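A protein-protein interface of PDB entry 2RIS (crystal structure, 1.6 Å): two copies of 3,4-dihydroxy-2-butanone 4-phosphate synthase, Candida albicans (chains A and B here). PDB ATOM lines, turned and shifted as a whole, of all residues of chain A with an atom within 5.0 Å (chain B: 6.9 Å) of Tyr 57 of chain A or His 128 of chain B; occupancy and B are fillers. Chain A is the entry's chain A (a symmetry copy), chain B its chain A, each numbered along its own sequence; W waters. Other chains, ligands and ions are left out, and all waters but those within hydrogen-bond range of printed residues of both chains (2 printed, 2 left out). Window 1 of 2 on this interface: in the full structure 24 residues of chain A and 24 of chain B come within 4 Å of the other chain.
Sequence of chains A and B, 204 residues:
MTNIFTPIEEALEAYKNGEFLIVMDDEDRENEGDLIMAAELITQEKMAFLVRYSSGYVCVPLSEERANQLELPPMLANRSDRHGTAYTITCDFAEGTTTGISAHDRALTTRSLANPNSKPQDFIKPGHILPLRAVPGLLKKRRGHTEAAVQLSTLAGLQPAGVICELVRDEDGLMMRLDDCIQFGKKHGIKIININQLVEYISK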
ATOM      1  N   SER A  55      -9.594 -15.444  33.518  1.00  0.00           N
ATOM      2  CA  SER A  55     -10.361 -14.755  32.483  1.00  0.00           C
ATOM      3  C   SER A  55     -11.870 -14.781  32.769  1.00  0.00           C
ATOM      4  O   SER A  55     -12.620 -13.985  32.209  1.00  0.00           O
ATOM      5  CB  SER A  55     -10.118 -15.408  31.123  1.00  0.00           C
ATOM      6  OG  SER A  55     -10.894 -16.591  31.022  1.00  0.00           O
ATOM      7  N   GLY A  56     -12.304 -15.723  33.606  1.00  0.00           N
ATOM      8  CA  GLY A  56     -13.729 -15.894  33.930  1.00  0.00           C
ATOM      9  C   GLY A  56     -14.513 -16.648  32.872  1.00  0.00           C
ATOM     10  O   GLY A  56     -15.681 -16.946  33.067  1.00  0.00           O
ATOM     11  N   TYR A  57     -13.876 -16.956  31.743  1.00  0.00           N
ATOM     12  CA  TYR A  57     -14.534 -17.738  30.700  1.00  0.00           C
ATOM     13  C   TYR A  57     -14.378 -19.202  31.096  1.00  0.00           C
ATOM     14  O   TYR A  57     -13.553 -19.932  30.532  1.00  0.00           O
ATOM     15  CB  TYR A  57     -13.879 -17.429  29.348  1.00  0.00           C
ATOM     16  CG  TYR A  57     -14.746 -17.640  28.118  1.00  0.00           C
ATOM     17  CD1 TYR A  57     -15.897 -16.885  27.912  1.00  0.00           C
ATOM     18  CD2 TYR A  57     -14.391 -18.580  27.141  1.00  0.00           C
ATOM     19  CE1 TYR A  57     -16.684 -17.064  26.756  1.00  0.00           C
ATOM     20  CE2 TYR A  57     -15.172 -18.768  25.990  1.00  0.00           C
ATOM     21  CZ  TYR A  57     -16.320 -18.001  25.808  1.00  0.00           C
ATOM     22  OH  TYR A  57     -17.118 -18.153  24.687  1.00  0.00           O
ATOM     23  N   VAL A  58     -15.169 -19.617  32.089  1.00  0.00           N
ATOM     24  CA  VAL A  58     -14.959 -20.898  32.767  1.00  0.00           C
ATOM     25  C   VAL A  58     -15.561 -22.037  31.965  1.00  0.00           C
ATOM     26  O   VAL A  58     -16.765 -22.030  31.656  1.00  0.00           O
ATOM     27  CB  VAL A  58     -15.527 -20.883  34.215  1.00  0.00           C
ATOM     28  CG1 VAL A  58     -15.404 -22.258  34.858  1.00  0.00           C
ATOM     29  CG2 VAL A  58     -14.809 -19.826  35.081  1.00  0.00           C
ATOM     30  N   CYS A  59     -14.704 -23.013  31.669  1.00  0.00           N
ATOM     31  CA  CYS A  59     -15.031 -24.156  30.823  1.00  0.00           C
ATOM     32  C   CYS A  59     -14.985 -25.462  31.610  1.00  0.00           C
ATOM     33  O   CYS A  59     -14.233 -25.595  32.576  1.00  0.00           O
ATOM     34  CB  CYS A  59     -14.055 -24.231  29.656  1.00  0.00           C
ATOM     35  SG  CYS A  59     -14.175 -22.844  28.515  1.00  0.00           S
ATOM     36  N   TYR A  87     -16.143 -26.507  21.879  1.00  0.00           N
ATOM     37  CA  TYR A  87     -17.248 -26.016  22.702  1.00  0.00           C
ATOM     38  C   TYR A  87     -18.547 -26.721  22.358  1.00  0.00           C
ATOM     39  O   TYR A  87     -18.830 -26.961  21.178  1.00  0.00           O
ATOM     40  CB  TYR A  87     -17.477 -24.527  22.462  1.00  0.00           C
ATOM     41  CG  TYR A  87     -16.332 -23.640  22.847  1.00  0.00           C
ATOM     42  CD1 TYR A  87     -15.468 -23.142  21.875  1.00  0.00           C
ATOM     43  CD2 TYR A  87     -16.122 -23.277  24.179  1.00  0.00           C
ATOM     44  CE1 TYR A  87     -14.408 -22.309  22.218  1.00  0.00           C
ATOM     45  CE2 TYR A  87     -15.060 -22.446  24.536  1.00  0.00           C
ATOM     46  CZ  TYR A  87     -14.211 -21.967  23.547  1.00  0.00           C
ATOM     47  OH  TYR A  87     -13.160 -21.139  23.880  1.00  0.00           O
ATOM     48  N   LEU A 130     -19.442 -23.310  29.973  1.00  0.00           N
ATOM     49  CA  LEU A 130     -18.982 -23.749  28.652  1.00  0.00           C
ATOM     50  C   LEU A 130     -18.380 -25.159  28.703  1.00  0.00           C
ATOM     51  O   LEU A 130     -17.185 -25.299  28.960  1.00  0.00           O
ATOM     52  CB  LEU A 130     -17.923 -22.772  28.120  1.00  0.00           C
ATOM     53  CG  LEU A 130     -18.369 -21.319  27.891  1.00  0.00           C
ATOM     54  CD1 LEU A 130     -17.393 -20.349  28.555  1.00  0.00           C
ATOM     55  CD2 LEU A 130     -18.527 -21.002  26.415  1.00  0.00           C
ATOM     56  N   ILE A 164     -11.777 -25.599  34.090  1.00  0.00           N
ATOM     57  CA  ILE A 164     -10.542 -24.905  33.722  1.00  0.00           C
ATOM     58  C   ILE A 164     -10.769 -23.430  33.437  1.00  0.00           C
ATOM     59  O   ILE A 164     -11.854 -23.023  33.010  1.00  0.00           O
ATOM     60  CB  ILE A 164      -9.864 -25.549  32.471  1.00  0.00           C
ATOM     61  CG1 ILE A 164     -10.677 -25.300  31.190  1.00  0.00           C
ATOM     62  CG2 ILE A 164      -9.605 -27.045  32.686  1.00  0.00           C
ATOM     63  CD1 ILE A 164     -10.019 -25.856  29.906  1.00  0.00           C
ATOM     64  N   CYS A 165      -9.729 -22.637  33.675  1.00  0.00           N
ATOM     65  CA  CYS A 165      -9.733 -21.246  33.234  1.00  0.00           C
ATOM     66  C   CYS A 165      -8.320 -20.683  33.272  1.00  0.00           C
ATOM     67  O   CYS A 165      -7.465 -21.170  34.014  1.00  0.00           O
ATOM     68  CB  CYS A 165     -10.706 -20.407  34.074  1.00  0.00           C
ATOM     69  SG  CYS A 165     -11.334 -18.955  33.206  1.00  0.00           S
ATOM     70  N   GLU A 166      -8.088 -19.664  32.453  1.00  0.00           N
ATOM     71  CA  GLU A 166      -6.752 -19.103  32.239  1.00  0.00           C
ATOM     72  C   GLU A 166      -6.375 -18.109  33.315  1.00  0.00           C
ATOM     73  O   GLU A 166      -7.129 -17.170  33.579  1.00  0.00           O
ATOM     74  CB  GLU A 166      -6.687 -18.371  30.890  1.00  0.00           C
ATOM     75  CG  GLU A 166      -7.093 -19.181  29.675  1.00  0.00           C
ATOM     76  CD  GLU A 166      -8.589 -19.161  29.367  1.00  0.00           C
ATOM     77  OE1 GLU A 166      -9.393 -18.640  30.172  1.00  0.00           O
ATOM     78  OE2 GLU A 166      -8.949 -19.680  28.288  1.00  0.00           O
ATOM     79  N   VAL B  51     -12.806  -7.389  32.914  1.00  0.00           N
ATOM     80  CA  VAL B  51     -12.589  -8.775  33.329  1.00  0.00           C
ATOM     81  C   VAL B  51     -12.137  -8.847  34.786  1.00  0.00           C
ATOM     82  O   VAL B  51     -12.605  -9.687  35.551  1.00  0.00           O
ATOM     83  CB  VAL B  51     -11.574  -9.462  32.390  1.00  0.00           C
ATOM     84  CG1 VAL B  51     -11.127 -10.803  32.945  1.00  0.00           C
ATOM     85  CG2 VAL B  51     -12.200  -9.632  31.008  1.00  0.00           C
ATOM     86  N   SER B  55     -17.501 -11.129  36.443  1.00  0.00           N
ATOM     87  CA  SER B  55     -17.594 -12.578  36.274  1.00  0.00           C
ATOM     88  C   SER B  55     -16.689 -13.085  35.141  1.00  0.00           C
ATOM     89  O   SER B  55     -16.384 -14.274  35.079  1.00  0.00           O
ATOM     90  CB  SER B  55     -19.034 -12.981  35.958  1.00  0.00           C
ATOM     91  OG  SER B  55     -19.306 -12.723  34.590  1.00  0.00           O
ATOM     92  N   GLY B  56     -16.306 -12.187  34.234  1.00  0.00           N
ATOM     93  CA  GLY B  56     -15.480 -12.546  33.070  1.00  0.00           C
ATOM     94  C   GLY B  56     -16.263 -13.175  31.933  1.00  0.00           C
ATOM     95  O   GLY B  56     -15.714 -13.424  30.870  1.00  0.00           O
ATOM     96  N   TYR B  57     -17.551 -13.442  32.150  1.00  0.00           N
ATOM     97  CA  TYR B  57     -18.395 -13.986  31.090  1.00  0.00           C
ATOM     98  C   TYR B  57     -18.862 -12.797  30.259  1.00  0.00           C
ATOM     99  O   TYR B  57     -20.012 -12.354  30.366  1.00  0.00           O
ATOM    100  CB  TYR B  57     -19.566 -14.750  31.719  1.00  0.00           C
ATOM    101  CG  TYR B  57     -20.183 -15.849  30.871  1.00  0.00           C
ATOM    102  CD1 TYR B  57     -19.445 -16.970  30.498  1.00  0.00           C
ATOM    103  CD2 TYR B  57     -21.523 -15.779  30.468  1.00  0.00           C
ATOM    104  CE1 TYR B  57     -20.028 -18.001  29.734  1.00  0.00           C
ATOM    105  CE2 TYR B  57     -22.110 -16.800  29.702  1.00  0.00           C
ATOM    106  CZ  TYR B  57     -21.350 -17.909  29.340  1.00  0.00           C
ATOM    107  OH  TYR B  57     -21.890 -18.938  28.589  1.00  0.00           O
ATOM    108  N   VAL B  58     -17.945 -12.271  29.441  1.00  0.00           N
ATOM    109  CA  VAL B  58     -18.140 -10.977  28.784  1.00  0.00           C
ATOM    110  C   VAL B  58     -18.998 -11.126  27.541  1.00  0.00           C
ATOM    111  O   VAL B  58     -18.665 -11.903  26.629  1.00  0.00           O
ATOM    112  CB  VAL B  58     -16.785 -10.296  28.440  1.00  0.00           C
ATOM    113  CG1 VAL B  58     -17.009  -9.011  27.653  1.00  0.00           C
ATOM    114  CG2 VAL B  58     -15.972 -10.001  29.718  1.00  0.00           C
ATOM    115  N   THR B  90     -20.893 -18.090  19.743  1.00  0.00           N
ATOM    116  CA  THR B  90     -19.774 -17.243  20.175  1.00  0.00           C
ATOM    117  C   THR B  90     -18.803 -16.999  19.021  1.00  0.00           C
ATOM    118  O   THR B  90     -18.846 -17.696  18.010  1.00  0.00           O
ATOM    119  CB  THR B  90     -19.036 -17.880  21.360  1.00  0.00           C
ATOM    120  OG1 THR B  90     -18.558 -19.179  20.974  1.00  0.00           O
ATOM    121  CG2 THR B  90     -19.975 -18.012  22.554  1.00  0.00           C
ATOM    122  N   CYS B  91     -17.927 -16.007  19.169  1.00  0.00           N
ATOM    123  CA  CYS B  91     -17.030 -15.673  18.073  1.00  0.00           C
ATOM    124  C   CYS B  91     -15.763 -14.941  18.502  1.00  0.00           C
ATOM    125  O   CYS B  91     -15.713 -14.349  19.582  1.00  0.00           O
ATOM    126  CB  CYS B  91     -17.784 -14.825  17.041  1.00  0.00           C
ATOM    127  SG  CYS B  91     -18.237 -13.165  17.648  1.00  0.00           S
ATOM    128  N   ASP B  92     -14.756 -15.019  17.635  1.00  0.00           N
ATOM    129  CA  ASP B  92     -13.543 -14.196  17.704  1.00  0.00           C
ATOM    130  C   ASP B  92     -13.330 -13.534  16.345  1.00  0.00           C
ATOM    131  O   ASP B  92     -13.564 -14.149  15.304  1.00  0.00           O
ATOM    132  CB  ASP B  92     -12.309 -15.059  17.993  1.00  0.00           C
ATOM    133  CG  ASP B  92     -12.326 -15.674  19.375  1.00  0.00           C
ATOM    134  OD1 ASP B  92     -11.792 -16.796  19.504  1.00  0.00           O
ATOM    135  OD2 ASP B  92     -12.861 -15.046  20.309  1.00  0.00           O
ATOM    136  N   THR B  98      -5.036 -14.173  18.518  1.00  0.00           N
ATOM    137  CA  THR B  98      -4.363 -15.462  18.639  1.00  0.00           C
ATOM    138  C   THR B  98      -5.211 -16.411  19.486  1.00  0.00           C
ATOM    139  O   THR B  98      -5.928 -17.259  18.949  1.00  0.00           O
ATOM    140  CB  THR B  98      -2.949 -15.316  19.256  1.00  0.00           C
ATOM    141  OG1 THR B  98      -3.015 -14.516  20.442  1.00  0.00           O
ATOM    142  CG2 THR B  98      -1.980 -14.665  18.259  1.00  0.00           C
ATOM    143  N   THR B  99      -5.151 -16.244  20.806  1.00  0.00           N
ATOM    144  CA  THR B  99      -5.897 -17.106  21.730  1.00  0.00           C
ATOM    145  C   THR B  99      -7.386 -16.760  21.790  1.00  0.00           C
ATOM    146  O   THR B  99      -8.205 -17.586  22.212  1.00  0.00           O
ATOM    147  CB  THR B  99      -5.341 -17.018  23.177  1.00  0.00           C
ATOM    148  OG1 THR B  99      -5.488 -15.677  23.666  1.00  0.00           O
ATOM    149  CG2 THR B  99      -3.861 -17.424  23.244  1.00  0.00           C
ATOM    150  N   GLY B 100      -7.728 -15.535  21.399  1.00  0.00           N
ATOM    151  CA  GLY B 100      -9.109 -15.070  21.448  1.00  0.00           C
ATOM    152  C   GLY B 100      -9.537 -14.592  22.829  1.00  0.00           C
ATOM    153  O   GLY B 100     -10.408 -13.734  22.947  1.00  0.00           O
ATOM    154  N   ILE B 101      -8.920 -15.138  23.875  1.00  0.00           N
ATOM    155  CA  ILE B 101      -9.364 -14.905  25.252  1.00  0.00           C
ATOM    156  C   ILE B 101      -8.622 -13.741  25.938  1.00  0.00           C
ATOM    157  O   ILE B 101      -9.092 -13.190  26.953  1.00  0.00           O
ATOM    158  CB  ILE B 101      -9.302 -16.230  26.093  1.00  0.00           C
ATOM    159  CG1 ILE B 101      -9.972 -16.087  27.472  1.00  0.00           C
ATOM    160  CG2 ILE B 101      -7.861 -16.719  26.238  1.00  0.00           C
ATOM    161  CD1 ILE B 101     -11.458 -15.785  27.434  1.00  0.00           C
ATOM    162  N   SER B 102      -7.469 -13.359  25.391  1.00  0.00           N
ATOM    163  CA  SER B 102      -6.721 -12.237  25.959  1.00  0.00           C
ATOM    164  C   SER B 102      -7.577 -10.972  25.997  1.00  0.00           C
ATOM    165  O   SER B 102      -8.507 -10.810  25.204  1.00  0.00           O
ATOM    166  CB  SER B 102      -5.440 -11.979  25.170  1.00  0.00           C
ATOM    167  OG  SER B 102      -5.735 -11.456  23.885  1.00  0.00           O
ATOM    168  N   ARG B 106     -10.260 -10.061  23.098  1.00  0.00           N
ATOM    169  CA  ARG B 106     -11.675  -9.821  23.406  1.00  0.00           C
ATOM    170  C   ARG B 106     -12.100  -8.384  23.102  1.00  0.00           C
ATOM    171  O   ARG B 106     -13.202  -8.150  22.597  1.00  0.00           O
ATOM    172  CB  ARG B 106     -12.030 -10.229  24.841  1.00  0.00           C
ATOM    173  CG  ARG B 106     -12.114 -11.731  25.002  1.00  0.00           C
ATOM    174  CD  ARG B 106     -12.974 -12.118  26.176  1.00  0.00           C
ATOM    175  NE  ARG B 106     -12.205 -12.177  27.422  1.00  0.00           N
ATOM    176  CZ  ARG B 106     -12.698 -12.630  28.576  1.00  0.00           C
ATOM    177  NH1 ARG B 106     -13.969 -13.033  28.657  1.00  0.00           N
ATOM    178  NH2 ARG B 106     -11.924 -12.672  29.659  1.00  0.00           N
ATOM    179  N   THR B 109     -12.282  -8.102  19.235  1.00  0.00           N
ATOM    180  CA  THR B 109     -13.501  -8.742  18.754  1.00  0.00           C
ATOM    181  C   THR B 109     -14.724  -7.871  19.032  1.00  0.00           C
ATOM    182  O   THR B 109     -15.571  -7.665  18.154  1.00  0.00           O
ATOM    183  CB  THR B 109     -13.659 -10.117  19.380  1.00  0.00           C
ATOM    184  OG1 THR B 109     -12.559 -10.940  18.956  1.00  0.00           O
ATOM    185  CG2 THR B 109     -14.987 -10.756  18.970  1.00  0.00           C
ATOM    186  N   ILE B 124     -14.321 -15.897  13.416  1.00  0.00           N
ATOM    187  CA  ILE B 124     -14.243 -17.333  13.668  1.00  0.00           C
ATOM    188  C   ILE B 124     -15.313 -17.691  14.686  1.00  0.00           C
ATOM    189  O   ILE B 124     -15.488 -16.998  15.694  1.00  0.00           O
ATOM    190  CB  ILE B 124     -12.848 -17.771  14.199  1.00  0.00           C
ATOM    191  CG1 ILE B 124     -11.730 -17.369  13.228  1.00  0.00           C
ATOM    192  CG2 ILE B 124     -12.801 -19.290  14.411  1.00  0.00           C
ATOM    193  CD1 ILE B 124     -10.369 -17.258  13.888  1.00  0.00           C
ATOM    194  N   PRO B 126     -16.981 -21.261  16.759  1.00  0.00           N
ATOM    195  CA  PRO B 126     -17.159 -20.494  18.004  1.00  0.00           C
ATOM    196  C   PRO B 126     -15.906 -19.701  18.388  1.00  0.00           C
ATOM    197  O   PRO B 126     -14.854 -19.838  17.762  1.00  0.00           O
ATOM    198  CB  PRO B 126     -17.431 -21.591  19.045  1.00  0.00           C
ATOM    199  CG  PRO B 126     -16.733 -22.800  18.490  1.00  0.00           C
ATOM    200  CD  PRO B 126     -16.958 -22.717  17.013  1.00  0.00           C
ATOM    201  N   GLY B 127     -16.029 -18.865  19.411  1.00  0.00           N
ATOM    202  CA  GLY B 127     -14.903 -18.095  19.901  1.00  0.00           C
ATOM    203  C   GLY B 127     -15.045 -17.771  21.369  1.00  0.00           C
ATOM    204  O   GLY B 127     -15.594 -18.561  22.129  1.00  0.00           O
ATOM    205  N   HIS B 128     -14.577 -16.589  21.755  1.00  0.00           N
ATOM    206  CA  HIS B 128     -14.438 -16.245  23.168  1.00  0.00           C
ATOM    207  C   HIS B 128     -15.244 -15.023  23.593  1.00  0.00           C
ATOM    208  O   HIS B 128     -15.198 -14.633  24.773  1.00  0.00           O
ATOM    209  CB  HIS B 128     -12.960 -16.080  23.522  1.00  0.00           C
ATOM    210  CG  HIS B 128     -12.156 -17.329  23.319  1.00  0.00           C
ATOM    211  ND1 HIS B 128     -11.690 -17.718  22.082  1.00  0.00           N
ATOM    212  CD2 HIS B 128     -11.734 -18.271  24.196  1.00  0.00           C
ATOM    213  CE1 HIS B 128     -11.024 -18.854  22.203  1.00  0.00           C
ATOM    214  NE2 HIS B 128     -11.033 -19.209  23.476  1.00  0.00           N
ATOM    215  N   ILE B 129     -15.990 -14.438  22.648  1.00  0.00           N
ATOM    216  CA  ILE B 129     -16.977 -13.397  22.965  1.00  0.00           C
ATOM    217  C   ILE B 129     -18.390 -13.941  22.794  1.00  0.00           C
ATOM    218  O   ILE B 129     -18.652 -14.711  21.864  1.00  0.00           O
ATOM    219  CB  ILE B 129     -16.754 -12.113  22.109  1.00  0.00           C
ATOM    220  CG1 ILE B 129     -15.616 -11.272  22.695  1.00  0.00           C
ATOM    221  CG2 ILE B 129     -18.030 -11.278  21.967  1.00  0.00           C
ATOM    222  CD1 ILE B 129     -15.913 -10.590  24.007  1.00  0.00           C
ATOM    223  N   LEU B 130     -19.284 -13.533  23.697  1.00  0.00           N
ATOM    224  CA  LEU B 130     -20.694 -13.932  23.686  1.00  0.00           C
ATOM    225  C   LEU B 130     -21.602 -12.793  23.207  1.00  0.00           C
ATOM    226  O   LEU B 130     -22.031 -11.977  24.023  1.00  0.00           O
ATOM    227  CB  LEU B 130     -21.124 -14.355  25.099  1.00  0.00           C
ATOM    228  CG  LEU B 130     -20.403 -15.563  25.715  1.00  0.00           C
ATOM    229  CD1 LEU B 130     -19.902 -15.230  27.119  1.00  0.00           C
ATOM    230  CD2 LEU B 130     -21.285 -16.799  25.734  1.00  0.00           C
HETATM  231  O   HOH W   1     -17.361 -20.509  23.084  1.00  0.00           O
HETATM  232  O   HOH W   2     -11.703 -21.144  26.051  1.00  0.00           O
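Of the 10 printed residues of chain A, 6 touch a printed residue of chain B.
Hydrophobic or aromatic side chains of chain A that line the printed part of chain B: Tyr 57, Tyr 87 and Leu 130.
Of the 21 printed residues of chain B, 11 touch a printed residue of chain A.
Printed residues of chain B that touch a printed residue of chain A: Val 51, Ser 55, Gly 56, Tyr 57, Thr 90, Ile 101, Arg 106, Pro 126, Gly 127, His 128 and Leu 130.
Among the printed residues, 16 pairs touch across the chains.
Among the printed residues, no Asp or Glu carboxylate lies within 4 Å of a Lys or Arg side-chain nitrogen of the other chain.
O of Ser 55 of chain A touches CG1 of Val 51 of chain B, at 3.6 Å.
CG1 of Ile 101 of chain B touches OG of Ser 55 of chain A (3.7 Å).
Gly 56 of chain B touches Gly 56 of chain A.
Thr 90 of chain B touches Tyr 57 of chain A.
Ile 101 of chain B touches Tyr 57 of chain A (CD1 to CB, 3.5 Å).
Leu 130 of chain B touches Tyr 57 of chain A.
Tyr 87 of chain A touches Pro 126 of chain B (CD1 to CG, 3.6 Å).
Gly 127 of chain B touches Tyr 87 of chain A (O to CE1, 3.9 Å).
CD1 of Leu 130 of chain A touches CE1 of Tyr 57 of chain B, at 3.7 Å.
Glu 166 of chain A touches Ile 101 of chain B (OE1 to CG1, 3.8 Å).
The side-chain hydroxyl (OG) of Ser 55 of chain A sits at hydrogen-bond distance from the backbone NH (N) of Tyr 57 of chain A, 3.1 Å away.
SG of Cys 165 of chain A lies within hydrogen-bond range of OG of Ser 55 of chain A, 3.2 Å away.
A ring nitrogen (ND1) of His 128 of chain B lies close to the backbone carbonyl oxygen (O) of Thr 99 of chain B, at 3.5 Å.
The side-chain carboxylate (OE1) of Glu 166 of chain A lies within hydrogen-bond range of the side-chain sulfur (SG) of Cys 165 of chain A.
The backbone NH (N) of Tyr 57 of chain A sits at hydrogen-bond distance from the side-chain sulfur (SG) of Cys 165 of chain A (3.5 Å).
OD2 of Asp 92 of chain B lies within hydrogen-bond range of N of His 128 of chain B, 2.7 Å away.
Tyr 57 of chain A touches five residues of chain B.
His 128 of chain B touches just these residues of chain A: Tyr 57 (3.5 Å) and Tyr 87 (2.9 Å).
Printed residues of chain B within 4 Å of Tyr 87 of chain A: Pro 126 (3.6 Å), Gly 127 (3.9 Å) and His 128 (2.9 Å).
Of the printed residues of chain B, Glu 166 of chain A touches Ile 101.
Printed residues of chain A within 4 Å of Ile 101 of chain B: Ser 55, Tyr 57 and Glu 166.
Val 58 of chain B touches none of the printed residues of chain A.
Thr 98 of chain B touches none of the printed residues of chain A.
Ser 55 of chain A touches Gly 56 of chain B, and with the chains exchanged Gly 56 of chain A touches Ser 55 of chain B.
Gly 56 of chain A touches its own counterpart, Gly 56 of chain B.
Tyr 57 of chain A touches Leu 130 of chain B, and with the chains exchanged Leu 130 of chain A touches Tyr 57 of chain B.
Of the 16 pairs that touch across the chains among the printed residues, 5 have their exchanged pair printed and touching as well.
A ring nitrogen (NE2) of His 128 of chain B sits at hydrogen-bond distance from the side-chain hydroxyl (OH) of Tyr 87 of chain A (2.9 Å).
O of Gly 56 of chain B sits close to O of Ser 55 of chain A, at 3.4 Å.
The backbone carbonyl oxygen of Gly 56 of chain A sits close to the backbone carbonyl oxygen of Ser 55 of chain B, at 3.4 Å.
The side-chain hydroxyl (OH) of Tyr 57 of chain A sits at hydrogen-bond distance from the backbone carbonyl oxygen (O) of Gly 127 of chain B (3.0 Å).
The guanidinium group (NH2) of Arg 106 of chain B lies within hydrogen-bond range of the backbone carbonyl oxygen (O) of Ser 55 of chain A (3.0 Å).
Water W2 bridges the side-chain hydroxyl of Tyr 87 of chain A (2.6 Å) and a ring nitrogen (NE2) of His 128 of chain B (3.3 Å).
Water W1 lies within hydrogen-bond range of the side-chain hydroxyl (OG1) of Thr 90 of chain B (2.8 Å), the backbone carbonyl oxygen (O) of Gly 127 of chain B (2.8 Å) and the side-chain hydroxyl (OH) of Tyr 57 of chain A (2.9 Å).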
